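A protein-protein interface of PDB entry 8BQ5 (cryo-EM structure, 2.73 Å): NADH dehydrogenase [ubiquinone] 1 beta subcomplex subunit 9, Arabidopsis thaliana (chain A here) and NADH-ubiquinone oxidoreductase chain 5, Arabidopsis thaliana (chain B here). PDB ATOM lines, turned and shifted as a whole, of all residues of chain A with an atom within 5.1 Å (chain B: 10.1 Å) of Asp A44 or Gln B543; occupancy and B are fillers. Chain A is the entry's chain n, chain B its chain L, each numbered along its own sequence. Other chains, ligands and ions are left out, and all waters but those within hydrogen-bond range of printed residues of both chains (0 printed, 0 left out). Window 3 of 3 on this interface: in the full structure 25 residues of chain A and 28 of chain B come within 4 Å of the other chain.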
ATOM      1  N   THR A  31     -14.398 -14.107  -0.350  1.00  0.00           N
ATOM      2  CA  THR A  31     -15.536 -14.658   0.378  1.00  0.00           C
ATOM      3  C   THR A  31     -16.455 -13.552   0.882  1.00  0.00           C
ATOM      4  O   THR A  31     -17.683 -13.666   0.796  1.00  0.00           O
ATOM      5  CB  THR A  31     -15.046 -15.521   1.541  1.00  0.00           C
ATOM      6  OG1 THR A  31     -14.504 -16.744   1.032  1.00  0.00           O
ATOM      7  CG2 THR A  31     -16.188 -15.842   2.495  1.00  0.00           C
ATOM      8  N   TRP A  34     -18.763 -11.969  -1.818  1.00  0.00           N
ATOM      9  CA  TRP A  34     -19.995 -12.737  -2.137  1.00  0.00           C
ATOM     10  C   TRP A  34     -21.011 -12.681  -0.990  1.00  0.00           C
ATOM     11  O   TRP A  34     -22.208 -12.611  -1.305  1.00  0.00           O
ATOM     12  CB  TRP A  34     -19.628 -14.186  -2.461  1.00  0.00           C
ATOM     13  CG  TRP A  34     -18.997 -14.413  -3.799  1.00  0.00           C
ATOM     14  CD1 TRP A  34     -17.699 -14.748  -4.044  1.00  0.00           C
ATOM     15  CD2 TRP A  34     -19.647 -14.369  -5.081  1.00  0.00           C
ATOM     16  NE1 TRP A  34     -17.491 -14.899  -5.387  1.00  0.00           N
ATOM     17  CE2 TRP A  34     -18.666 -14.671  -6.049  1.00  0.00           C
ATOM     18  CE3 TRP A  34     -20.950 -14.088  -5.509  1.00  0.00           C
ATOM     19  CZ2 TRP A  34     -18.951 -14.705  -7.413  1.00  0.00           C
ATOM     20  CZ3 TRP A  34     -21.227 -14.114  -6.857  1.00  0.00           C
ATOM     21  CH2 TRP A  34     -20.242 -14.423  -7.794  1.00  0.00           C
ATOM     22  N   ALA A  35     -20.568 -12.654   0.270  1.00  0.00           N
ATOM     23  CA  ALA A  35     -21.452 -12.756   1.425  1.00  0.00           C
ATOM     24  C   ALA A  35     -21.967 -11.411   1.914  1.00  0.00           C
ATOM     25  O   ALA A  35     -23.071 -11.343   2.463  1.00  0.00           O
ATOM     26  CB  ALA A  35     -20.736 -13.472   2.572  1.00  0.00           C
ATOM     27  N   ILE A  40     -23.181 -13.820   7.640  1.00  0.00           N
ATOM     28  CA  ILE A  40     -22.996 -14.848   6.624  1.00  0.00           C
ATOM     29  C   ILE A  40     -21.512 -15.118   6.431  1.00  0.00           C
ATOM     30  O   ILE A  40     -21.089 -16.270   6.292  1.00  0.00           O
ATOM     31  CB  ILE A  40     -23.670 -14.449   5.299  1.00  0.00           C
ATOM     32  CG1 ILE A  40     -25.107 -13.999   5.529  1.00  0.00           C
ATOM     33  CG2 ILE A  40     -23.715 -15.635   4.369  1.00  0.00           C
ATOM     34  CD1 ILE A  40     -25.757 -13.391   4.310  1.00  0.00           C
ATOM     35  N   PHE A  41     -20.697 -14.060   6.475  1.00  0.00           N
ATOM     36  CA  PHE A  41     -19.270 -14.188   6.202  1.00  0.00           C
ATOM     37  C   PHE A  41     -18.583 -15.102   7.209  1.00  0.00           C
ATOM     38  O   PHE A  41     -17.639 -15.818   6.857  1.00  0.00           O
ATOM     39  CB  PHE A  41     -18.620 -12.805   6.206  1.00  0.00           C
ATOM     40  CG  PHE A  41     -17.119 -12.837   6.181  1.00  0.00           C
ATOM     41  CD1 PHE A  41     -16.446 -13.389   5.105  1.00  0.00           C
ATOM     42  CD2 PHE A  41     -16.382 -12.311   7.228  1.00  0.00           C
ATOM     43  CE1 PHE A  41     -15.065 -13.420   5.075  1.00  0.00           C
ATOM     44  CE2 PHE A  41     -15.000 -12.340   7.203  1.00  0.00           C
ATOM     45  CZ  PHE A  41     -14.342 -12.896   6.125  1.00  0.00           C
ATOM     46  N   TYR A  42     -19.040 -15.091   8.465  1.00  0.00           N
ATOM     47  CA  TYR A  42     -18.386 -15.879   9.505  1.00  0.00           C
ATOM     48  C   TYR A  42     -18.357 -17.358   9.139  1.00  0.00           C
ATOM     49  O   TYR A  42     -17.310 -18.009   9.203  1.00  0.00           O
ATOM     50  CB  TYR A  42     -19.096 -15.691  10.846  1.00  0.00           C
ATOM     51  CG  TYR A  42     -19.207 -14.268  11.333  1.00  0.00           C
ATOM     52  CD1 TYR A  42     -18.237 -13.321  11.036  1.00  0.00           C
ATOM     53  CD2 TYR A  42     -20.286 -13.877  12.109  1.00  0.00           C
ATOM     54  CE1 TYR A  42     -18.351 -12.022  11.493  1.00  0.00           C
ATOM     55  CE2 TYR A  42     -20.409 -12.589  12.566  1.00  0.00           C
ATOM     56  CZ  TYR A  42     -19.442 -11.664  12.260  1.00  0.00           C
ATOM     57  OH  TYR A  42     -19.579 -10.378  12.727  1.00  0.00           O
ATOM     58  N   ARG A  43     -19.510 -17.908   8.753  1.00  0.00           N
ATOM     59  CA  ARG A  43     -19.546 -19.322   8.405  1.00  0.00           C
ATOM     60  C   ARG A  43     -18.775 -19.590   7.123  1.00  0.00           C
ATOM     61  O   ARG A  43     -17.927 -20.485   7.083  1.00  0.00           O
ATOM     62  CB  ARG A  43     -20.989 -19.817   8.297  1.00  0.00           C
ATOM     63  CG  ARG A  43     -21.965 -19.089   9.204  1.00  0.00           C
ATOM     64  CD  ARG A  43     -23.300 -19.831   9.295  1.00  0.00           C
ATOM     65  NE  ARG A  43     -23.976 -19.988   8.010  1.00  0.00           N
ATOM     66  CZ  ARG A  43     -24.341 -18.993   7.212  1.00  0.00           C
ATOM     67  NH1 ARG A  43     -24.157 -17.729   7.550  1.00  0.00           N
ATOM     68  NH2 ARG A  43     -24.922 -19.276   6.050  1.00  0.00           N
ATOM     69  N   ASP A  44     -19.014 -18.797   6.077  1.00  0.00           N
ATOM     70  CA  ASP A  44     -18.304 -19.016   4.821  1.00  0.00           C
ATOM     71  C   ASP A  44     -16.796 -18.882   5.007  1.00  0.00           C
ATOM     72  O   ASP A  44     -16.015 -19.487   4.264  1.00  0.00           O
ATOM     73  CB  ASP A  44     -18.815 -18.055   3.748  1.00  0.00           C
ATOM     74  CG  ASP A  44     -20.307 -17.799   3.857  1.00  0.00           C
ATOM     75  OD1 ASP A  44     -20.719 -16.622   3.792  1.00  0.00           O
ATOM     76  OD2 ASP A  44     -21.066 -18.775   4.029  1.00  0.00           O
ATOM     77  N   ALA A  45     -16.370 -18.106   6.008  1.00  0.00           N
ATOM     78  CA  ALA A  45     -14.949 -18.020   6.332  1.00  0.00           C
ATOM     79  C   ALA A  45     -14.428 -19.328   6.912  1.00  0.00           C
ATOM     80  O   ALA A  45     -13.294 -19.734   6.631  1.00  0.00           O
ATOM     81  CB  ALA A  45     -14.702 -16.872   7.309  1.00  0.00           C
ATOM     82  N   SER A  46     -15.233 -19.995   7.743  1.00  0.00           N
ATOM     83  CA  SER A  46     -14.773 -21.223   8.386  1.00  0.00           C
ATOM     84  C   SER A  46     -14.666 -22.367   7.387  1.00  0.00           C
ATOM     85  O   SER A  46     -13.709 -23.148   7.429  1.00  0.00           O
ATOM     86  CB  SER A  46     -15.707 -21.593   9.537  1.00  0.00           C
ATOM     87  OG  SER A  46     -15.518 -20.718  10.635  1.00  0.00           O
ATOM     88  N   ASP A  47     -15.636 -22.482   6.477  1.00  0.00           N
ATOM     89  CA  ASP A  47     -15.592 -23.547   5.480  1.00  0.00           C
ATOM     90  C   ASP A  47     -14.377 -23.412   4.573  1.00  0.00           C
ATOM     91  O   ASP A  47     -13.778 -24.418   4.176  1.00  0.00           O
ATOM     92  CB  ASP A  47     -16.883 -23.551   4.662  1.00  0.00           C
ATOM     93  CG  ASP A  47     -18.073 -24.035   5.463  1.00  0.00           C
ATOM     94  OD1 ASP A  47     -17.876 -24.629   6.542  1.00  0.00           O
ATOM     95  OD2 ASP A  47     -19.210 -23.775   5.036  1.00  0.00           O
ATOM     96  N   LEU A  48     -13.999 -22.177   4.230  1.00  0.00           N
ATOM     97  CA  LEU A  48     -12.832 -21.971   3.377  1.00  0.00           C
ATOM     98  C   LEU A  48     -11.543 -22.314   4.120  1.00  0.00           C
ATOM     99  O   LEU A  48     -10.655 -22.971   3.564  1.00  0.00           O
ATOM    100  CB  LEU A  48     -12.811 -20.528   2.856  1.00  0.00           C
ATOM    101  CG  LEU A  48     -11.489 -19.839   2.505  1.00  0.00           C
ATOM    102  CD1 LEU A  48     -10.969 -20.425   1.234  1.00  0.00           C
ATOM    103  CD2 LEU A  48     -11.679 -18.380   2.248  1.00  0.00           C
ATOM    104  N   LEU B 303     -27.651  -6.124  -9.609  1.00  0.00           N
ATOM    105  CA  LEU B 303     -26.418  -6.709  -9.025  1.00  0.00           C
ATOM    106  C   LEU B 303     -25.376  -5.606  -8.794  1.00  0.00           C
ATOM    107  O   LEU B 303     -24.300  -5.932  -8.269  1.00  0.00           O
ATOM    108  CB  LEU B 303     -25.889  -7.822  -9.937  1.00  0.00           C
ATOM    109  CG  LEU B 303     -26.803  -9.039 -10.071  1.00  0.00           C
ATOM    110  CD1 LEU B 303     -26.194 -10.077 -10.996  1.00  0.00           C
ATOM    111  CD2 LEU B 303     -27.097  -9.648  -8.711  1.00  0.00           C
ATOM    112  N   ARG B 366     -21.889  -2.711  -0.050  1.00  0.00           N
ATOM    113  CA  ARG B 366     -21.468  -3.929   0.691  1.00  0.00           C
ATOM    114  C   ARG B 366     -20.577  -3.523   1.868  1.00  0.00           C
ATOM    115  O   ARG B 366     -20.147  -4.425   2.606  1.00  0.00           O
ATOM    116  CB  ARG B 366     -20.740  -4.909  -0.234  1.00  0.00           C
ATOM    117  CG  ARG B 366     -21.580  -5.425  -1.391  1.00  0.00           C
ATOM    118  CD  ARG B 366     -20.707  -6.219  -2.339  1.00  0.00           C
ATOM    119  NE  ARG B 366     -19.741  -5.344  -2.983  1.00  0.00           N
ATOM    120  CZ  ARG B 366     -18.792  -5.749  -3.813  1.00  0.00           C
ATOM    121  NH1 ARG B 366     -18.668  -7.031  -4.104  1.00  0.00           N
ATOM    122  NH2 ARG B 366     -17.970  -4.866  -4.351  1.00  0.00           N
ATOM    123  N   LEU B 440     -29.966  -2.071   2.019  1.00  0.00           N
ATOM    124  CA  LEU B 440     -28.540  -2.306   2.229  1.00  0.00           C
ATOM    125  C   LEU B 440     -27.830  -1.064   2.753  1.00  0.00           C
ATOM    126  O   LEU B 440     -26.782  -1.171   3.399  1.00  0.00           O
ATOM    127  CB  LEU B 440     -27.889  -2.777   0.929  1.00  0.00           C
ATOM    128  CG  LEU B 440     -28.220  -4.196   0.468  1.00  0.00           C
ATOM    129  CD1 LEU B 440     -27.506  -4.512  -0.835  1.00  0.00           C
ATOM    130  CD2 LEU B 440     -27.853  -5.203   1.542  1.00  0.00           C
ATOM    131  N   VAL B 535     -34.305 -11.548  -0.049  1.00  0.00           N
ATOM    132  CA  VAL B 535     -32.945 -11.879  -0.463  1.00  0.00           C
ATOM    133  C   VAL B 535     -31.919 -11.176   0.420  1.00  0.00           C
ATOM    134  O   VAL B 535     -30.869 -11.742   0.744  1.00  0.00           O
ATOM    135  CB  VAL B 535     -32.746 -11.546  -1.954  1.00  0.00           C
ATOM    136  CG1 VAL B 535     -31.274 -11.529  -2.307  1.00  0.00           C
ATOM    137  CG2 VAL B 535     -33.477 -12.557  -2.816  1.00  0.00           C
ATOM    138  N   ASN B 536     -32.205  -9.944   0.831  1.00  0.00           N
ATOM    139  CA  ASN B 536     -31.229  -9.118   1.527  1.00  0.00           C
ATOM    140  C   ASN B 536     -31.251  -9.286   3.042  1.00  0.00           C
ATOM    141  O   ASN B 536     -30.336  -8.797   3.714  1.00  0.00           O
ATOM    142  CB  ASN B 536     -31.442  -7.646   1.174  1.00  0.00           C
ATOM    143  CG  ASN B 536     -31.526  -7.415  -0.317  1.00  0.00           C
ATOM    144  OD1 ASN B 536     -31.625  -8.359  -1.100  1.00  0.00           O
ATOM    145  ND2 ASN B 536     -31.493  -6.154  -0.718  1.00  0.00           N
ATOM    146  N   LEU B 537     -32.261  -9.949   3.605  1.00  0.00           N
ATOM    147  CA  LEU B 537     -32.349  -9.970   5.061  1.00  0.00           C
ATOM    148  C   LEU B 537     -32.695 -11.336   5.647  1.00  0.00           C
ATOM    149  O   LEU B 537     -32.481 -11.563   6.843  1.00  0.00           O
ATOM    150  CB  LEU B 537     -33.371  -8.928   5.524  1.00  0.00           C
ATOM    151  CG  LEU B 537     -32.802  -7.572   5.958  1.00  0.00           C
ATOM    152  CD1 LEU B 537     -33.835  -6.466   5.801  1.00  0.00           C
ATOM    153  CD2 LEU B 537     -32.290  -7.624   7.390  1.00  0.00           C
ATOM    154  N   VAL B 538     -33.223 -12.257   4.839  1.00  0.00           N
ATOM    155  CA  VAL B 538     -33.584 -13.575   5.360  1.00  0.00           C
ATOM    156  C   VAL B 538     -32.921 -14.667   4.529  1.00  0.00           C
ATOM    157  O   VAL B 538     -33.162 -15.860   4.746  1.00  0.00           O
ATOM    158  CB  VAL B 538     -35.114 -13.774   5.415  1.00  0.00           C
ATOM    159  CG1 VAL B 538     -35.813 -12.525   5.940  1.00  0.00           C
ATOM    160  CG2 VAL B 538     -35.674 -14.185   4.060  1.00  0.00           C
ATOM    161  N   ALA B 539     -32.065 -14.274   3.588  1.00  0.00           N
ATOM    162  CA  ALA B 539     -31.378 -15.249   2.752  1.00  0.00           C
ATOM    163  C   ALA B 539     -29.893 -15.220   3.076  1.00  0.00           C
ATOM    164  O   ALA B 539     -29.281 -14.147   3.089  1.00  0.00           O
ATOM    165  CB  ALA B 539     -31.608 -14.965   1.265  1.00  0.00           C
ATOM    166  N   ASP B 540     -29.319 -16.397   3.336  1.00  0.00           N
ATOM    167  CA  ASP B 540     -27.903 -16.513   3.645  1.00  0.00           C
ATOM    168  C   ASP B 540     -27.202 -17.609   2.856  1.00  0.00           C
ATOM    169  O   ASP B 540     -25.971 -17.699   2.915  1.00  0.00           O
ATOM    170  CB  ASP B 540     -27.701 -16.751   5.150  1.00  0.00           C
ATOM    171  CG  ASP B 540     -28.392 -18.007   5.646  1.00  0.00           C
ATOM    172  OD1 ASP B 540     -28.330 -18.270   6.865  1.00  0.00           O
ATOM    173  OD2 ASP B 540     -28.994 -18.733   4.828  1.00  0.00           O
ATOM    174  N   GLN B 541     -27.944 -18.453   2.134  1.00  0.00           N
ATOM    175  CA  GLN B 541     -27.301 -19.385   1.214  1.00  0.00           C
ATOM    176  C   GLN B 541     -27.798 -19.248  -0.220  1.00  0.00           C
ATOM    177  O   GLN B 541     -27.709 -20.224  -0.976  1.00  0.00           O
ATOM    178  CB  GLN B 541     -27.478 -20.832   1.685  1.00  0.00           C
ATOM    179  CG  GLN B 541     -26.545 -21.215   2.817  1.00  0.00           C
ATOM    180  CD  GLN B 541     -25.508 -22.228   2.379  1.00  0.00           C
ATOM    181  OE1 GLN B 541     -25.787 -23.104   1.559  1.00  0.00           O
ATOM    182  NE2 GLN B 541     -24.298 -22.107   2.913  1.00  0.00           N
ATOM    183  N   PHE B 542     -28.313 -18.091  -0.626  1.00  0.00           N
ATOM    184  CA  PHE B 542     -28.656 -17.842  -2.024  1.00  0.00           C
ATOM    185  C   PHE B 542     -27.446 -17.366  -2.820  1.00  0.00           C
ATOM    186  O   PHE B 542     -27.569 -16.842  -3.930  1.00  0.00           O
ATOM    187  CB  PHE B 542     -29.800 -16.830  -2.082  1.00  0.00           C
ATOM    188  CG  PHE B 542     -30.422 -16.685  -3.441  1.00  0.00           C
ATOM    189  CD1 PHE B 542     -31.109 -17.740  -4.022  1.00  0.00           C
ATOM    190  CD2 PHE B 542     -30.344 -15.485  -4.127  1.00  0.00           C
ATOM    191  CE1 PHE B 542     -31.690 -17.604  -5.270  1.00  0.00           C
ATOM    192  CE2 PHE B 542     -30.923 -15.344  -5.373  1.00  0.00           C
ATOM    193  CZ  PHE B 542     -31.597 -16.404  -5.945  1.00  0.00           C
ATOM    194  N   GLN B 543     -26.255 -17.557  -2.257  1.00  0.00           N
ATOM    195  CA  GLN B 543     -25.013 -17.087  -2.854  1.00  0.00           C
ATOM    196  C   GLN B 543     -24.075 -18.261  -3.089  1.00  0.00           C
ATOM    197  O   GLN B 543     -23.018 -18.111  -3.708  1.00  0.00           O
ATOM    198  CB  GLN B 543     -24.353 -16.056  -1.942  1.00  0.00           C
ATOM    199  CG  GLN B 543     -24.007 -16.618  -0.577  1.00  0.00           C
ATOM    200  CD  GLN B 543     -23.578 -15.551   0.400  1.00  0.00           C
ATOM    201  OE1 GLN B 543     -23.979 -14.395   0.291  1.00  0.00           O
ATOM    202  NE2 GLN B 543     -22.748 -15.933   1.359  1.00  0.00           N
ATOM    203  N   ARG B 544     -24.449 -19.432  -2.569  1.00  0.00           N
ATOM    204  CA  ARG B 544     -23.657 -20.631  -2.808  1.00  0.00           C
ATOM    205  C   ARG B 544     -23.787 -21.102  -4.249  1.00  0.00           C
ATOM    206  O   ARG B 544     -22.829 -21.637  -4.815  1.00  0.00           O
ATOM    207  CB  ARG B 544     -24.077 -21.732  -1.834  1.00  0.00           C
ATOM    208  CG  ARG B 544     -23.301 -23.033  -1.970  1.00  0.00           C
ATOM    209  CD  ARG B 544     -23.760 -24.075  -0.949  1.00  0.00           C
ATOM    210  NE  ARG B 544     -23.033 -25.335  -1.056  1.00  0.00           N
ATOM    211  CZ  ARG B 544     -23.357 -26.324  -1.878  1.00  0.00           C
ATOM    212  NH1 ARG B 544     -24.388 -26.229  -2.701  1.00  0.00           N
ATOM    213  NH2 ARG B 544     -22.624 -27.435  -1.878  1.00  0.00           N
ATOM    214  N   ALA B 545     -24.958 -20.902  -4.860  1.00  0.00           N
ATOM    215  CA  ALA B 545     -25.145 -21.310  -6.249  1.00  0.00           C
ATOM    216  C   ALA B 545     -24.211 -20.547  -7.178  1.00  0.00           C
ATOM    217  O   ALA B 545     -23.716 -21.100  -8.167  1.00  0.00           O
ATOM    218  CB  ALA B 545     -26.603 -21.111  -6.664  1.00  0.00           C
ATOM    219  N   PHE B 546     -23.946 -19.276  -6.872  1.00  0.00           N
ATOM    220  CA  PHE B 546     -23.013 -18.488  -7.666  1.00  0.00           C
ATOM    221  C   PHE B 546     -21.565 -18.918  -7.485  1.00  0.00           C
ATOM    222  O   PHE B 546     -20.710 -18.484  -8.263  1.00  0.00           O
ATOM    223  CB  PHE B 546     -23.156 -17.007  -7.320  1.00  0.00           C
ATOM    224  CG  PHE B 546     -24.569 -16.517  -7.352  1.00  0.00           C
ATOM    225  CD1 PHE B 546     -25.403 -16.853  -8.404  1.00  0.00           C
ATOM    226  CD2 PHE B 546     -25.066 -15.723  -6.334  1.00  0.00           C
ATOM    227  CE1 PHE B 546     -26.704 -16.406  -8.442  1.00  0.00           C
ATOM    228  CE2 PHE B 546     -26.368 -15.273  -6.368  1.00  0.00           C
ATOM    229  CZ  PHE B 546     -27.188 -15.615  -7.422  1.00  0.00           C
ATOM    230  N   GLN B 547     -21.269 -19.754  -6.490  1.00  0.00           N
ATOM    231  CA  GLN B 547     -19.903 -20.169  -6.212  1.00  0.00           C
ATOM    232  C   GLN B 547     -19.612 -21.621  -6.564  1.00  0.00           C
ATOM    233  O   GLN B 547     -18.437 -22.005  -6.595  1.00  0.00           O
ATOM    234  CB  GLN B 547     -19.565 -19.933  -4.733  1.00  0.00           C
ATOM    235  CG  GLN B 547     -19.046 -18.540  -4.441  1.00  0.00           C
ATOM    236  CD  GLN B 547     -18.147 -18.500  -3.225  1.00  0.00           C
ATOM    237  OE1 GLN B 547     -17.143 -19.207  -3.156  1.00  0.00           O
ATOM    238  NE2 GLN B 547     -18.500 -17.664  -2.257  1.00  0.00           N
ATOM    239  N   THR B 548     -20.635 -22.439  -6.822  1.00  0.00           N
ATOM    240  CA  THR B 548     -20.436 -23.830  -7.206  1.00  0.00           C
ATOM    241  C   THR B 548     -20.953 -24.177  -8.591  1.00  0.00           C
ATOM    242  O   THR B 548     -20.482 -25.160  -9.173  1.00  0.00           O
ATOM    243  CB  THR B 548     -21.112 -24.781  -6.206  1.00  0.00           C
ATOM    244  OG1 THR B 548     -22.468 -25.004  -6.607  1.00  0.00           O
ATOM    245  CG2 THR B 548     -21.078 -24.214  -4.800  1.00  0.00           C
ATOM    246  N   SER B 549     -21.901 -23.419  -9.130  1.00  0.00           N
ATOM    247  CA  SER B 549     -22.486 -23.700 -10.433  1.00  0.00           C
ATOM    248  C   SER B 549     -21.893 -22.757 -11.466  1.00  0.00           C
ATOM    249  O   SER B 549     -21.895 -21.537 -11.272  1.00  0.00           O
ATOM    250  CB  SER B 549     -24.008 -23.553 -10.398  1.00  0.00           C
ATOM    251  OG  SER B 549     -24.556 -23.744 -11.689  1.00  0.00           O
ATOM    252  N   CYS B 552     -24.849 -20.592 -12.921  1.00  0.00           N
ATOM    253  CA  CYS B 552     -25.279 -19.555 -11.990  1.00  0.00           C
ATOM    254  C   CYS B 552     -24.183 -18.522 -11.772  1.00  0.00           C
ATOM    255  O   CYS B 552     -24.471 -17.337 -11.565  1.00  0.00           O
ATOM    256  CB  CYS B 552     -25.703 -20.182 -10.663  1.00  0.00           C
ATOM    257  SG  CYS B 552     -27.420 -20.738 -10.624  1.00  0.00           S
ATOM    258  N   ASN B 553     -22.921 -18.954 -11.790  1.00  0.00           N
ATOM    259  CA  ASN B 553     -21.814 -18.004 -11.746  1.00  0.00           C
ATOM    260  C   ASN B 553     -21.798 -17.127 -12.989  1.00  0.00           C
ATOM    261  O   ASN B 553     -21.617 -15.907 -12.899  1.00  0.00           O
ATOM    262  CB  ASN B 553     -20.488 -18.749 -11.606  1.00  0.00           C
ATOM    263  CG  ASN B 553     -19.339 -17.831 -11.244  1.00  0.00           C
ATOM    264  OD1 ASN B 553     -18.575 -17.405 -12.109  1.00  0.00           O
ATOM    265  ND2 ASN B 553     -19.207 -17.529  -9.960  1.00  0.00           N
ATOM    266  N   TYR B 556     -24.704 -14.594 -13.036  1.00  0.00           N
ATOM    267  CA  TYR B 556     -24.420 -13.445 -12.184  1.00  0.00           C
ATOM    268  C   TYR B 556     -23.487 -12.465 -12.888  1.00  0.00           C
ATOM    269  O   TYR B 556     -23.687 -11.247 -12.830  1.00  0.00           O
ATOM    270  CB  TYR B 556     -23.830 -13.920 -10.850  1.00  0.00           C
ATOM    271  CG  TYR B 556     -23.514 -12.822  -9.852  1.00  0.00           C
ATOM    272  CD1 TYR B 556     -24.275 -12.668  -8.700  1.00  0.00           C
ATOM    273  CD2 TYR B 556     -22.427 -11.976 -10.030  1.00  0.00           C
ATOM    274  CE1 TYR B 556     -23.985 -11.678  -7.780  1.00  0.00           C
ATOM    275  CE2 TYR B 556     -22.134 -10.987  -9.122  1.00  0.00           C
ATOM    276  CZ  TYR B 556     -22.912 -10.842  -7.998  1.00  0.00           C
ATOM    277  OH  TYR B 556     -22.607  -9.855  -7.093  1.00  0.00           O
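CZ3 of Trp A34 touches CB of Phe B546 (3.5 Å).
Trp A34 touches Gln B547 (CD1 to NE2, 3.5 Å).
Trp A34 touches Asn B553.
Tyr B556 touches Trp A34 (CE1 to CZ3, 3.8 Å).
Ala A35 touches Gln B543 (CA to OE1, 3.2 Å).
Ile A40 touches Ala B539.
Ile A40 touches Asp B540.
Gln B543 touches Ile A40.
Of the printed residues of chain B, Ala A35 touches Gln B543 (3.2 Å).
Of the printed residues of chain B, Ile A40 touches Ala B539 (3.8 Å), Asp B540 (3.4 Å) and Gln B543 (3.2 Å).
Arg A43 touches one residue of chain B.
No residue of chain B comes within 4 Å of Ala A45.
No residue of chain B comes within 4 Å of Asp A47.
Printed residues of chain A within 4 Å of Asn B553: Trp A34 (3.8 Å).
Printed residues of chain A within 4 Å of Phe B546: Trp A34.
Printed residues of chain B within 4 Å of Trp A34: Gln B543, Phe B546, Gln B547, Asn B553 and Tyr B556.
Gln B541 touches none of the printed residues of chain A.
Tyr A42 touches none of the printed residues of chain B.
The nearest residue of chain B that does not touch Asp A44 is Gln B541 (4.8 Å).
The nearest printed residue of chain A that does not touch Ala B539 is Ala A35 (6.8 Å).
The backbone carbonyl oxygen (O) of Phe B546 sits at hydrogen-bond distance from the side-chain amide nitrogen (ND2) of Asn B553, 2.5 Å away.
OD1 of Asp A44 sits close to O of Ile A40 (2.6 Å).
Of the 12 printed residues of chain A, 5 touch a printed residue of chain B.
Printed residues of chain A that touch a printed residue of chain B: Trp A34, Ala A35, Ile A40, Arg A43 and Asp A44.
Hydrophobic or aromatic side chains of chain B within 4 Å of the printed part of chain A: Phe B546 and Tyr B556.
The side-chain carboxylate (OD1) of Asp B540 is in salt-bridge range of the guanidinium group (NH2) of Arg A43, 3.6 Å away.
The side-chain amide oxygen (OE1) of Gln B543 lies close to the backbone carbonyl oxygen (O) of Trp A34.
NE2 of Gln B543 is in hydrogen-bond range of OD1 of Asp A44 (3.2 Å).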
